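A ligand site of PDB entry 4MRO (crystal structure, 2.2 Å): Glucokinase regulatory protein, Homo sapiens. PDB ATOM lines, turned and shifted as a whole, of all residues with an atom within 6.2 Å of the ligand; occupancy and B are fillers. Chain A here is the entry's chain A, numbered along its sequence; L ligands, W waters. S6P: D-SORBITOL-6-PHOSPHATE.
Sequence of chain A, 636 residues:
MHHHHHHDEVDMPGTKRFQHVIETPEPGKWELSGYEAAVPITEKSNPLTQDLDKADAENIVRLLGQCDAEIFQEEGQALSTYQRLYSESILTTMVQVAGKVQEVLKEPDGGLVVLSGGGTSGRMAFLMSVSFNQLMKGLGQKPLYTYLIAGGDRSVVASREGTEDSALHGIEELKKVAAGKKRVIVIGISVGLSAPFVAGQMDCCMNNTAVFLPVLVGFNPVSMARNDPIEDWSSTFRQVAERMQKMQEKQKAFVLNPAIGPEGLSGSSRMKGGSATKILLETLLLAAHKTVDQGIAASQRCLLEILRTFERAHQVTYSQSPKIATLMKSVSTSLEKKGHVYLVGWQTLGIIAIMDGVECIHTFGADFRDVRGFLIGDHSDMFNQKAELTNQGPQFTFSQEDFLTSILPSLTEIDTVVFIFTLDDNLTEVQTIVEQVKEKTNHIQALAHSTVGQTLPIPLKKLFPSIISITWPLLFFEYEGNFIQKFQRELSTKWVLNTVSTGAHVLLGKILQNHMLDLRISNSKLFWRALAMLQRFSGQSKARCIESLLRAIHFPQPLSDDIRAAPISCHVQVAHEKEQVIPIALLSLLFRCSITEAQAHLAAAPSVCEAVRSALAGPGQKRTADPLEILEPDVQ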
ATOM      1  N   THR A  42     -13.934  -7.355  17.666  1.00  0.00           N
ATOM      2  CA  THR A  42     -14.556  -6.184  18.232  1.00  0.00           C
ATOM      3  C   THR A  42     -15.181  -6.453  19.589  1.00  0.00           C
ATOM      4  O   THR A  42     -15.411  -5.516  20.364  1.00  0.00           O
ATOM      5  CB  THR A  42     -15.629  -5.614  17.283  1.00  0.00           C
ATOM      6  OG1 THR A  42     -16.635  -6.600  16.950  1.00  0.00           O
ATOM      7  CG2 THR A  42     -14.975  -5.146  16.015  1.00  0.00           C
ATOM      8  N   GLY A 118     -25.489   2.595  12.343  1.00  0.00           N
ATOM      9  CA  GLY A 118     -26.264   2.649  13.586  1.00  0.00           C
ATOM     10  C   GLY A 118     -25.432   3.283  14.688  1.00  0.00           C
ATOM     11  O   GLY A 118     -24.186   3.157  14.636  1.00  0.00           O
ATOM     12  N   GLY A 119     -26.089   3.906  15.681  1.00  0.00           N
ATOM     13  CA  GLY A 119     -25.420   4.367  16.916  1.00  0.00           C
ATOM     14  C   GLY A 119     -24.227   5.239  16.491  1.00  0.00           C
ATOM     15  O   GLY A 119     -24.353   6.124  15.581  1.00  0.00           O
ATOM     16  N   THR A 120     -23.048   4.932  17.056  1.00  0.00           N
ATOM     17  CA  THR A 120     -21.886   5.766  16.859  1.00  0.00           C
ATOM     18  C   THR A 120     -21.386   5.727  15.472  1.00  0.00           C
ATOM     19  O   THR A 120     -20.779   6.678  15.029  1.00  0.00           O
ATOM     20  CB  THR A 120     -20.780   5.381  17.780  1.00  0.00           C
ATOM     21  OG1 THR A 120     -21.320   5.324  19.103  1.00  0.00           O
ATOM     22  CG2 THR A 120     -19.683   6.392  17.734  1.00  0.00           C
ATOM     23  N   SER A 121     -21.635   4.650  14.735  1.00  0.00           N
ATOM     24  CA  SER A 121     -21.306   4.655  13.334  1.00  0.00           C
ATOM     25  C   SER A 121     -22.178   5.661  12.647  1.00  0.00           C
ATOM     26  O   SER A 121     -21.736   6.322  11.699  1.00  0.00           O
ATOM     27  CB  SER A 121     -21.512   3.272  12.730  1.00  0.00           C
ATOM     28  OG  SER A 121     -20.583   2.367  13.327  1.00  0.00           O
ATOM     29  N   GLY A 122     -23.441   5.795  13.103  1.00  0.00           N
ATOM     30  CA  GLY A 122     -24.373   6.796  12.535  1.00  0.00           C
ATOM     31  C   GLY A 122     -23.966   8.255  12.835  1.00  0.00           C
ATOM     32  O   GLY A 122     -23.980   9.118  11.946  1.00  0.00           O
ATOM     33  N   ARG A 123     -23.588   8.496  14.077  1.00  0.00           N
ATOM     34  CA  ARG A 123     -23.020   9.743  14.468  1.00  0.00           C
ATOM     35  C   ARG A 123     -21.785  10.173  13.641  1.00  0.00           C
ATOM     36  O   ARG A 123     -21.733  11.313  13.120  1.00  0.00           O
ATOM     37  CB  ARG A 123     -22.644   9.666  15.922  1.00  0.00           C
ATOM     38  CG  ARG A 123     -23.863   9.573  16.801  1.00  0.00           C
ATOM     39  CD  ARG A 123     -23.452   9.628  18.257  1.00  0.00           C
ATOM     40  NE  ARG A 123     -23.958   8.481  19.032  1.00  0.00           N
ATOM     41  CZ  ARG A 123     -25.217   8.353  19.468  1.00  0.00           C
ATOM     42  NH1 ARG A 123     -26.128   9.288  19.231  1.00  0.00           N
ATOM     43  NH2 ARG A 123     -25.562   7.295  20.170  1.00  0.00           N
ATOM     44  N   GLU A 161     -30.544   2.750  21.127  1.00  0.00           N
ATOM     45  CA  GLU A 161     -29.843   1.488  20.778  1.00  0.00           C
ATOM     46  C   GLU A 161     -30.703   0.413  20.052  1.00  0.00           C
ATOM     47  O   GLU A 161     -30.148  -0.425  19.338  1.00  0.00           O
ATOM     48  CB  GLU A 161     -29.267   0.879  22.045  1.00  0.00           C
ATOM     49  CG  GLU A 161     -28.080   1.645  22.613  1.00  0.00           C
ATOM     50  CD  GLU A 161     -26.847   1.438  21.791  1.00  0.00           C
ATOM     51  OE1 GLU A 161     -25.980   0.640  22.228  1.00  0.00           O
ATOM     52  OE2 GLU A 161     -26.760   2.068  20.717  1.00  0.00           O
ATOM     53  N   GLU A 164     -31.256  -0.215  15.538  1.00  0.00           N
ATOM     54  CA  GLU A 164     -30.343  -0.870  14.578  1.00  0.00           C
ATOM     55  C   GLU A 164     -30.751  -2.287  13.998  1.00  0.00           C
ATOM     56  O   GLU A 164     -30.075  -2.782  13.084  1.00  0.00           O
ATOM     57  CB  GLU A 164     -28.928  -0.896  15.180  1.00  0.00           C
ATOM     58  CG  GLU A 164     -28.644  -1.812  16.344  1.00  0.00           C
ATOM     59  CD  GLU A 164     -27.122  -2.026  16.567  1.00  0.00           C
ATOM     60  OE1 GLU A 164     -26.506  -1.080  17.121  1.00  0.00           O
ATOM     61  OE2 GLU A 164     -26.545  -3.112  16.215  1.00  0.00           O
ATOM     62  N   ILE A 189     -21.445   1.680   7.479  1.00  0.00           N
ATOM     63  CA  ILE A 189     -20.502   1.621   8.538  1.00  0.00           C
ATOM     64  C   ILE A 189     -20.990   0.768   9.686  1.00  0.00           C
ATOM     65  O   ILE A 189     -21.881   1.152  10.415  1.00  0.00           O
ATOM     66  CB  ILE A 189     -20.220   3.031   9.092  1.00  0.00           C
ATOM     67  CG1 ILE A 189     -19.760   3.940   7.933  1.00  0.00           C
ATOM     68  CG2 ILE A 189     -19.219   2.904  10.224  1.00  0.00           C
ATOM     69  CD1 ILE A 189     -19.654   5.431   8.280  1.00  0.00           C
ATOM     70  N   SER A 190     -20.335  -0.367   9.910  1.00  0.00           N
ATOM     71  CA  SER A 190     -20.654  -1.173  11.087  1.00  0.00           C
ATOM     72  C   SER A 190     -19.398  -1.827  11.620  1.00  0.00           C
ATOM     73  O   SER A 190     -18.858  -2.752  11.035  1.00  0.00           O
ATOM     74  CB  SER A 190     -21.730  -2.261  10.782  1.00  0.00           C
ATOM     75  OG  SER A 190     -22.125  -2.926  11.976  1.00  0.00           O
ATOM     76  N   VAL A 191     -18.978  -1.304  12.756  1.00  0.00           N
ATOM     77  CA  VAL A 191     -17.772  -1.630  13.377  1.00  0.00           C
ATOM     78  C   VAL A 191     -17.621  -3.102  13.543  1.00  0.00           C
ATOM     79  O   VAL A 191     -16.573  -3.691  13.202  1.00  0.00           O
ATOM     80  CB  VAL A 191     -17.666  -0.940  14.733  1.00  0.00           C
ATOM     81  CG1 VAL A 191     -16.442  -1.441  15.452  1.00  0.00           C
ATOM     82  CG2 VAL A 191     -17.479   0.560  14.521  1.00  0.00           C
ATOM     83  N   GLY A 192     -18.669  -3.709  14.072  1.00  0.00           N
ATOM     84  CA  GLY A 192     -18.683  -5.116  14.286  1.00  0.00           C
ATOM     85  C   GLY A 192     -19.030  -5.892  13.057  1.00  0.00           C
ATOM     86  O   GLY A 192     -19.025  -7.107  13.114  1.00  0.00           O
ATOM     87  N   LEU A 193     -19.291  -5.230  11.940  1.00  0.00           N
ATOM     88  CA  LEU A 193     -19.865  -5.905  10.767  1.00  0.00           C
ATOM     89  C   LEU A 193     -21.120  -6.711  11.258  1.00  0.00           C
ATOM     90  O   LEU A 193     -21.310  -7.924  11.039  1.00  0.00           O
ATOM     91  CB  LEU A 193     -18.840  -6.826  10.148  1.00  0.00           C
ATOM     92  CG  LEU A 193     -17.573  -6.244   9.506  1.00  0.00           C
ATOM     93  CD1 LEU A 193     -16.885  -7.310   8.648  1.00  0.00           C
ATOM     94  CD2 LEU A 193     -17.937  -5.083   8.623  1.00  0.00           C
ATOM     95  N   SER A 194     -21.962  -5.967  11.941  1.00  0.00           N
ATOM     96  CA  SER A 194     -22.976  -6.489  12.801  1.00  0.00           C
ATOM     97  C   SER A 194     -24.373  -5.945  12.483  1.00  0.00           C
ATOM     98  O   SER A 194     -25.289  -6.697  12.648  1.00  0.00           O
ATOM     99  CB  SER A 194     -22.647  -6.110  14.226  1.00  0.00           C
ATOM    100  OG  SER A 194     -23.844  -6.111  15.024  1.00  0.00           O
ATOM    101  N   ALA A 195     -24.546  -4.642  12.163  1.00  0.00           N
ATOM    102  CA  ALA A 195     -25.885  -4.024  12.337  1.00  0.00           C
ATOM    103  C   ALA A 195     -26.833  -4.373  11.156  1.00  0.00           C
ATOM    104  O   ALA A 195     -26.476  -4.217  10.003  1.00  0.00           O
ATOM    105  CB  ALA A 195     -25.783  -2.541  12.509  1.00  0.00           C
ATOM    106  N   VAL A 198     -27.406  -1.837   8.384  1.00  0.00           N
ATOM    107  CA  VAL A 198     -26.452  -1.761   7.259  1.00  0.00           C
ATOM    108  C   VAL A 198     -26.588  -2.937   6.360  1.00  0.00           C
ATOM    109  O   VAL A 198     -26.521  -2.807   5.148  1.00  0.00           O
ATOM    110  CB  VAL A 198     -25.005  -1.691   7.801  1.00  0.00           C
ATOM    111  CG1 VAL A 198     -23.980  -1.654   6.700  1.00  0.00           C
ATOM    112  CG2 VAL A 198     -24.890  -0.443   8.683  1.00  0.00           C
ATOM    113  N   GLY A 267     -16.166  -4.360  23.690  1.00  0.00           N
ATOM    114  CA  GLY A 267     -17.305  -4.231  22.851  1.00  0.00           C
ATOM    115  C   GLY A 267     -17.783  -2.806  22.839  1.00  0.00           C
ATOM    116  O   GLY A 267     -18.802  -2.534  22.268  1.00  0.00           O
ATOM    117  N   SER A 268     -17.063  -1.877  23.488  1.00  0.00           N
ATOM    118  CA  SER A 268     -17.522  -0.487  23.486  1.00  0.00           C
ATOM    119  C   SER A 268     -17.044   0.174  22.202  1.00  0.00           C
ATOM    120  O   SER A 268     -16.123   0.991  22.211  1.00  0.00           O
ATOM    121  CB  SER A 268     -17.064   0.276  24.725  1.00  0.00           C
ATOM    122  OG  SER A 268     -17.571   1.622  24.635  1.00  0.00           O
ATOM    123  N   SER A 269     -17.652  -0.202  21.085  1.00  0.00           N
ATOM    124  CA  SER A 269     -17.154   0.204  19.795  1.00  0.00           C
ATOM    125  C   SER A 269     -17.340   1.750  19.471  1.00  0.00           C
ATOM    126  O   SER A 269     -16.907   2.268  18.397  1.00  0.00           O
ATOM    127  CB  SER A 269     -17.792  -0.694  18.709  1.00  0.00           C
ATOM    128  OG  SER A 269     -19.135  -0.336  18.492  1.00  0.00           O
ATOM    129  N   ARG A 270     -17.954   2.494  20.379  1.00  0.00           N
ATOM    130  CA  ARG A 270     -17.990   3.946  20.172  1.00  0.00           C
ATOM    131  C   ARG A 270     -16.576   4.578  20.235  1.00  0.00           C
ATOM    132  O   ARG A 270     -16.398   5.678  19.783  1.00  0.00           O
ATOM    133  CB  ARG A 270     -18.860   4.611  21.248  1.00  0.00           C
ATOM    134  CG  ARG A 270     -18.209   4.575  22.621  1.00  0.00           C
ATOM    135  CD  ARG A 270     -19.206   4.953  23.681  1.00  0.00           C
ATOM    136  NE  ARG A 270     -18.533   5.341  24.931  1.00  0.00           N
ATOM    137  CZ  ARG A 270     -18.306   6.604  25.295  1.00  0.00           C
ATOM    138  NH1 ARG A 270     -18.740   7.643  24.540  1.00  0.00           N
ATOM    139  NH2 ARG A 270     -17.689   6.843  26.432  1.00  0.00           N
ATOM    140  N   MET A 271     -15.637   3.879  20.854  1.00  0.00           N
ATOM    141  CA  MET A 271     -14.311   4.342  21.124  1.00  0.00           C
ATOM    142  C   MET A 271     -13.395   4.144  19.941  1.00  0.00           C
ATOM    143  O   MET A 271     -13.477   4.888  18.987  1.00  0.00           O
ATOM    144  CB  MET A 271     -13.779   3.636  22.388  1.00  0.00           C
ATOM    145  CG  MET A 271     -14.531   4.033  23.652  1.00  0.00           C
ATOM    146  SD  MET A 271     -14.060   3.096  25.123  1.00  0.00           S
ATOM    147  CE  MET A 271     -12.871   4.340  25.705  1.00  0.00           C
ATOM    148  N   GLU A 359     -23.907   9.036  24.911  1.00  0.00           N
ATOM    149  CA  GLU A 359     -23.503   7.650  24.790  1.00  0.00           C
ATOM    150  C   GLU A 359     -23.224   7.054  26.143  1.00  0.00           C
ATOM    151  O   GLU A 359     -23.244   5.839  26.298  1.00  0.00           O
ATOM    152  CB  GLU A 359     -22.307   7.487  23.869  1.00  0.00           C
ATOM    153  CG  GLU A 359     -22.650   7.873  22.436  1.00  0.00           C
ATOM    154  CD  GLU A 359     -21.407   7.962  21.537  1.00  0.00           C
ATOM    155  OE1 GLU A 359     -20.286   7.958  22.098  1.00  0.00           O
ATOM    156  OE2 GLU A 359     -21.574   8.020  20.276  1.00  0.00           O
ATOM    157  N   HIS A 362     -26.490   4.646  27.594  1.00  0.00           N
ATOM    158  CA  HIS A 362     -26.523   3.213  27.292  1.00  0.00           C
ATOM    159  C   HIS A 362     -25.218   2.565  27.698  1.00  0.00           C
ATOM    160  O   HIS A 362     -25.238   1.502  28.259  1.00  0.00           O
ATOM    161  CB  HIS A 362     -26.899   2.917  25.858  1.00  0.00           C
ATOM    162  CG  HIS A 362     -26.068   3.595  24.813  1.00  0.00           C
ATOM    163  ND1 HIS A 362     -26.539   4.651  24.071  1.00  0.00           N
ATOM    164  CD2 HIS A 362     -24.839   3.324  24.342  1.00  0.00           C
ATOM    165  CE1 HIS A 362     -25.622   5.023  23.195  1.00  0.00           C
ATOM    166  NE2 HIS A 362     -24.567   4.246  23.358  1.00  0.00           N
ATOM    167  N   THR A 363     -24.083   3.239  27.566  1.00  0.00           N
ATOM    168  CA  THR A 363     -22.819   2.580  27.910  1.00  0.00           C
ATOM    169  C   THR A 363     -22.658   2.330  29.389  1.00  0.00           C
ATOM    170  O   THR A 363     -22.186   1.264  29.805  1.00  0.00           O
ATOM    171  CB  THR A 363     -21.613   3.377  27.403  1.00  0.00           C
ATOM    172  OG1 THR A 363     -21.790   3.672  26.010  1.00  0.00           O
ATOM    173  CG2 THR A 363     -20.356   2.587  27.585  1.00  0.00           C
ATOM    174  N   ASN A 523     -30.865  -4.225  22.289  1.00  0.00           N
ATOM    175  CA  ASN A 523     -30.835  -4.739  20.936  1.00  0.00           C
ATOM    176  C   ASN A 523     -30.289  -6.144  20.955  1.00  0.00           C
ATOM    177  O   ASN A 523     -29.728  -6.602  21.963  1.00  0.00           O
ATOM    178  CB  ASN A 523     -30.113  -3.778  19.961  1.00  0.00           C
ATOM    179  CG  ASN A 523     -28.651  -3.506  20.319  1.00  0.00           C
ATOM    180  OD1 ASN A 523     -28.090  -2.408  20.102  1.00  0.00           O
ATOM    181  ND2 ASN A 523     -27.994  -4.493  20.744  1.00  0.00           N
ATOM    182  N   LYS A 525     -27.738  -7.537  19.610  1.00  0.00           N
ATOM    183  CA  LYS A 525     -26.305  -7.629  19.887  1.00  0.00           C
ATOM    184  C   LYS A 525     -25.968  -7.590  21.410  1.00  0.00           C
ATOM    185  O   LYS A 525     -25.175  -8.397  21.928  1.00  0.00           O
ATOM    186  CB  LYS A 525     -25.536  -6.564  19.089  1.00  0.00           C
ATOM    187  CG  LYS A 525     -24.057  -6.497  19.435  1.00  0.00           C
ATOM    188  CD  LYS A 525     -23.294  -5.440  18.578  1.00  0.00           C
ATOM    189  CE  LYS A 525     -23.584  -4.009  19.007  1.00  0.00           C
ATOM    190  NZ  LYS A 525     -23.205  -3.147  17.891  1.00  0.00           N
ATOM    191  N   ARG A 529     -24.293 -10.231  23.913  1.00  0.00           N
ATOM    192  CA  ARG A 529     -23.180  -9.844  24.779  1.00  0.00           C
ATOM    193  C   ARG A 529     -23.507 -10.268  26.218  1.00  0.00           C
ATOM    194  O   ARG A 529     -22.662 -10.829  26.931  1.00  0.00           O
ATOM    195  CB  ARG A 529     -22.828  -8.345  24.702  1.00  0.00           C
ATOM    196  CG  ARG A 529     -21.520  -7.954  25.440  1.00  0.00           C
ATOM    197  CD  ARG A 529     -20.968  -6.600  24.991  1.00  0.00           C
ATOM    198  NE  ARG A 529     -20.949  -6.349  23.514  1.00  0.00           N
ATOM    199  CZ  ARG A 529     -21.264  -5.174  22.909  1.00  0.00           C
ATOM    200  NH1 ARG A 529     -21.684  -4.146  23.626  1.00  0.00           N
ATOM    201  NH2 ARG A 529     -21.202  -5.023  21.579  1.00  0.00           N
HETATM  202  C1  S6P L   1     -21.072   1.019  21.021  1.00  0.00           C
HETATM  203  C2  S6P L   1     -22.168   2.031  20.778  1.00  0.00           C
HETATM  204  C3  S6P L   1     -23.148   1.404  19.858  1.00  0.00           C
HETATM  205  C4  S6P L   1     -22.629   1.164  18.434  1.00  0.00           C
HETATM  206  C5  S6P L   1     -23.775   0.683  17.550  1.00  0.00           C
HETATM  207  C6  S6P L   1     -23.327   0.123  16.176  1.00  0.00           C
HETATM  208  O1  S6P L   1     -20.201   1.579  21.997  1.00  0.00           O
HETATM  209  O2  S6P L   1     -22.824   2.242  22.045  1.00  0.00           O
HETATM  210  O3  S6P L   1     -24.293   2.243  19.829  1.00  0.00           O
HETATM  211  O4  S6P L   1     -22.046   2.322  17.854  1.00  0.00           O
HETATM  212  O5  S6P L   1     -24.369  -0.431  18.233  1.00  0.00           O
HETATM  213  O6  S6P L   1     -22.182  -0.744  16.317  1.00  0.00           O
HETATM  214  P   S6P L   1     -21.698  -1.338  14.954  1.00  0.00           P
HETATM  215  O1P S6P L   1     -20.785  -2.452  15.197  1.00  0.00           O
HETATM  216  O2P S6P L   1     -22.813  -1.698  13.922  1.00  0.00           O
HETATM  217  O3P S6P L   1     -20.970  -0.079  14.355  1.00  0.00           O
HETATM  218  O   HOH W   1     -24.182  -3.464  15.414  1.00  0.00           O
HETATM  219  O   HOH W   2     -24.013   0.365  12.061  1.00  0.00           O
HETATM  220  O   HOH W   3     -19.986   1.247  16.600  1.00  0.00           O
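The side-chain hydroxyl of Ser 190 sits at hydrogen-bond distance from the backbone NH of Ala 195, at 3.0 Å.
The side-chain carboxylate (OE1) of Glu 359 is in salt-bridge range of the guanidinium group (NH1) of Arg 270, at 2.9 Å.
The backbone carbonyl oxygen of Glu 161 sits close to the side-chain amide oxygen of Asn 523 (3.0 Å).
The backbone carbonyl oxygen of Ile 189 lies close to the side-chain hydroxyl of Ser 121, at 3.4 Å.
OG of Ser 190 is in hydrogen-bond range of N of Ser 194.
The side-chain amino group (NZ) of Lys 525 lies within salt-bridge range of the side-chain carboxylate (OE2) of Glu 164.
The backbone NH of Lys 525 lies close to the side-chain amide nitrogen of Asn 523 (3.3 Å).
The side-chain hydroxyl (OG1) of Thr 120 lies within hydrogen-bond range of the side-chain carboxylate (OE2) of Glu 359 (3.0 Å).
An oxygen (O5) of the ligand sits at hydrogen-bond distance from the side-chain carboxylate (OE1) of Glu 164.
An oxygen (O1) of the ligand lies within hydrogen-bond range of the backbone NH of Ser 269, 3.2 Å away.
O4 of the ligand lies within hydrogen-bond range of N of Thr 120 (2.9 Å).
An oxygen (O3) of the ligand lies within hydrogen-bond range of the side-chain carboxylate of Glu 161 (2.6 Å).
An oxygen (O3P) of the ligand sits at hydrogen-bond distance from the backbone NH (N) of Val 191 (2.8 Å).
The side-chain hydroxyl (OG) of Ser 121 lies within hydrogen-bond range of an oxygen (O3P) of the ligand, 2.7 Å away.
N of Gly 192 sits at hydrogen-bond distance from O1P of the ligand (2.7 Å).
A ring nitrogen (NE2) of His 362 sits at hydrogen-bond distance from an oxygen (O2) of the ligand.
NZ of Lys 525 lies within salt-bridge range of O1P of the ligand (3.7 Å).
O1 of the ligand is in hydrogen-bond range of N of Arg 270 (2.9 Å).
The side-chain hydroxyl (OG1) of Thr 120 lies close to an oxygen (O4) of the ligand, 3.3 Å away.
The side-chain hydroxyl (OG) of Ser 190 lies within hydrogen-bond range of an oxygen (O2P) of the ligand.
O of Gly 118 touches C6 of the ligand (3.5 Å).
CA of Gly 119 touches O3 of the ligand (3.8 Å).
Ala 195 touches the ligand.
Ser 268 touches the ligand (C to O1, 3.5 Å).
Hydrophobic or aromatic side chains that line the ligand: Val 191, Ala 195 and His 362.
Within 4 Å of the ligand: Gly 118, Gly 119, Thr 120, Ser 121, Glu 161, Glu 164, Ser 190, Val 191, Gly 192, Ala 195, Ser 268, Ser 269, Arg 270, His 362 and Lys 525.
Along chain A the residues within 4 Å of the ligand span positions 118 to 525.
The nearest printed residue that does not touch the ligand is Ser 194 (4.2 Å).
Water W3 lies within hydrogen-bond range of the side-chain hydroxyl of Ser 269 (2.6 Å) and an oxygen (O4) of the ligand (2.6 Å).
Water W1 lies within hydrogen-bond range of OE2 of Glu 164 (2.5 Å), NZ of Lys 525 (2.7 Å), O2P of the ligand (2.7 Å), OG of Ser 194 (2.7 Å) and N of Ala 195 (3.5 Å).
Water W2 lies within hydrogen-bond range of the backbone NH of Gly 118 (2.7 Å), the backbone carbonyl oxygen of Ile 189 (2.8 Å) and an oxygen (O2P) of the ligand (3.0 Å).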
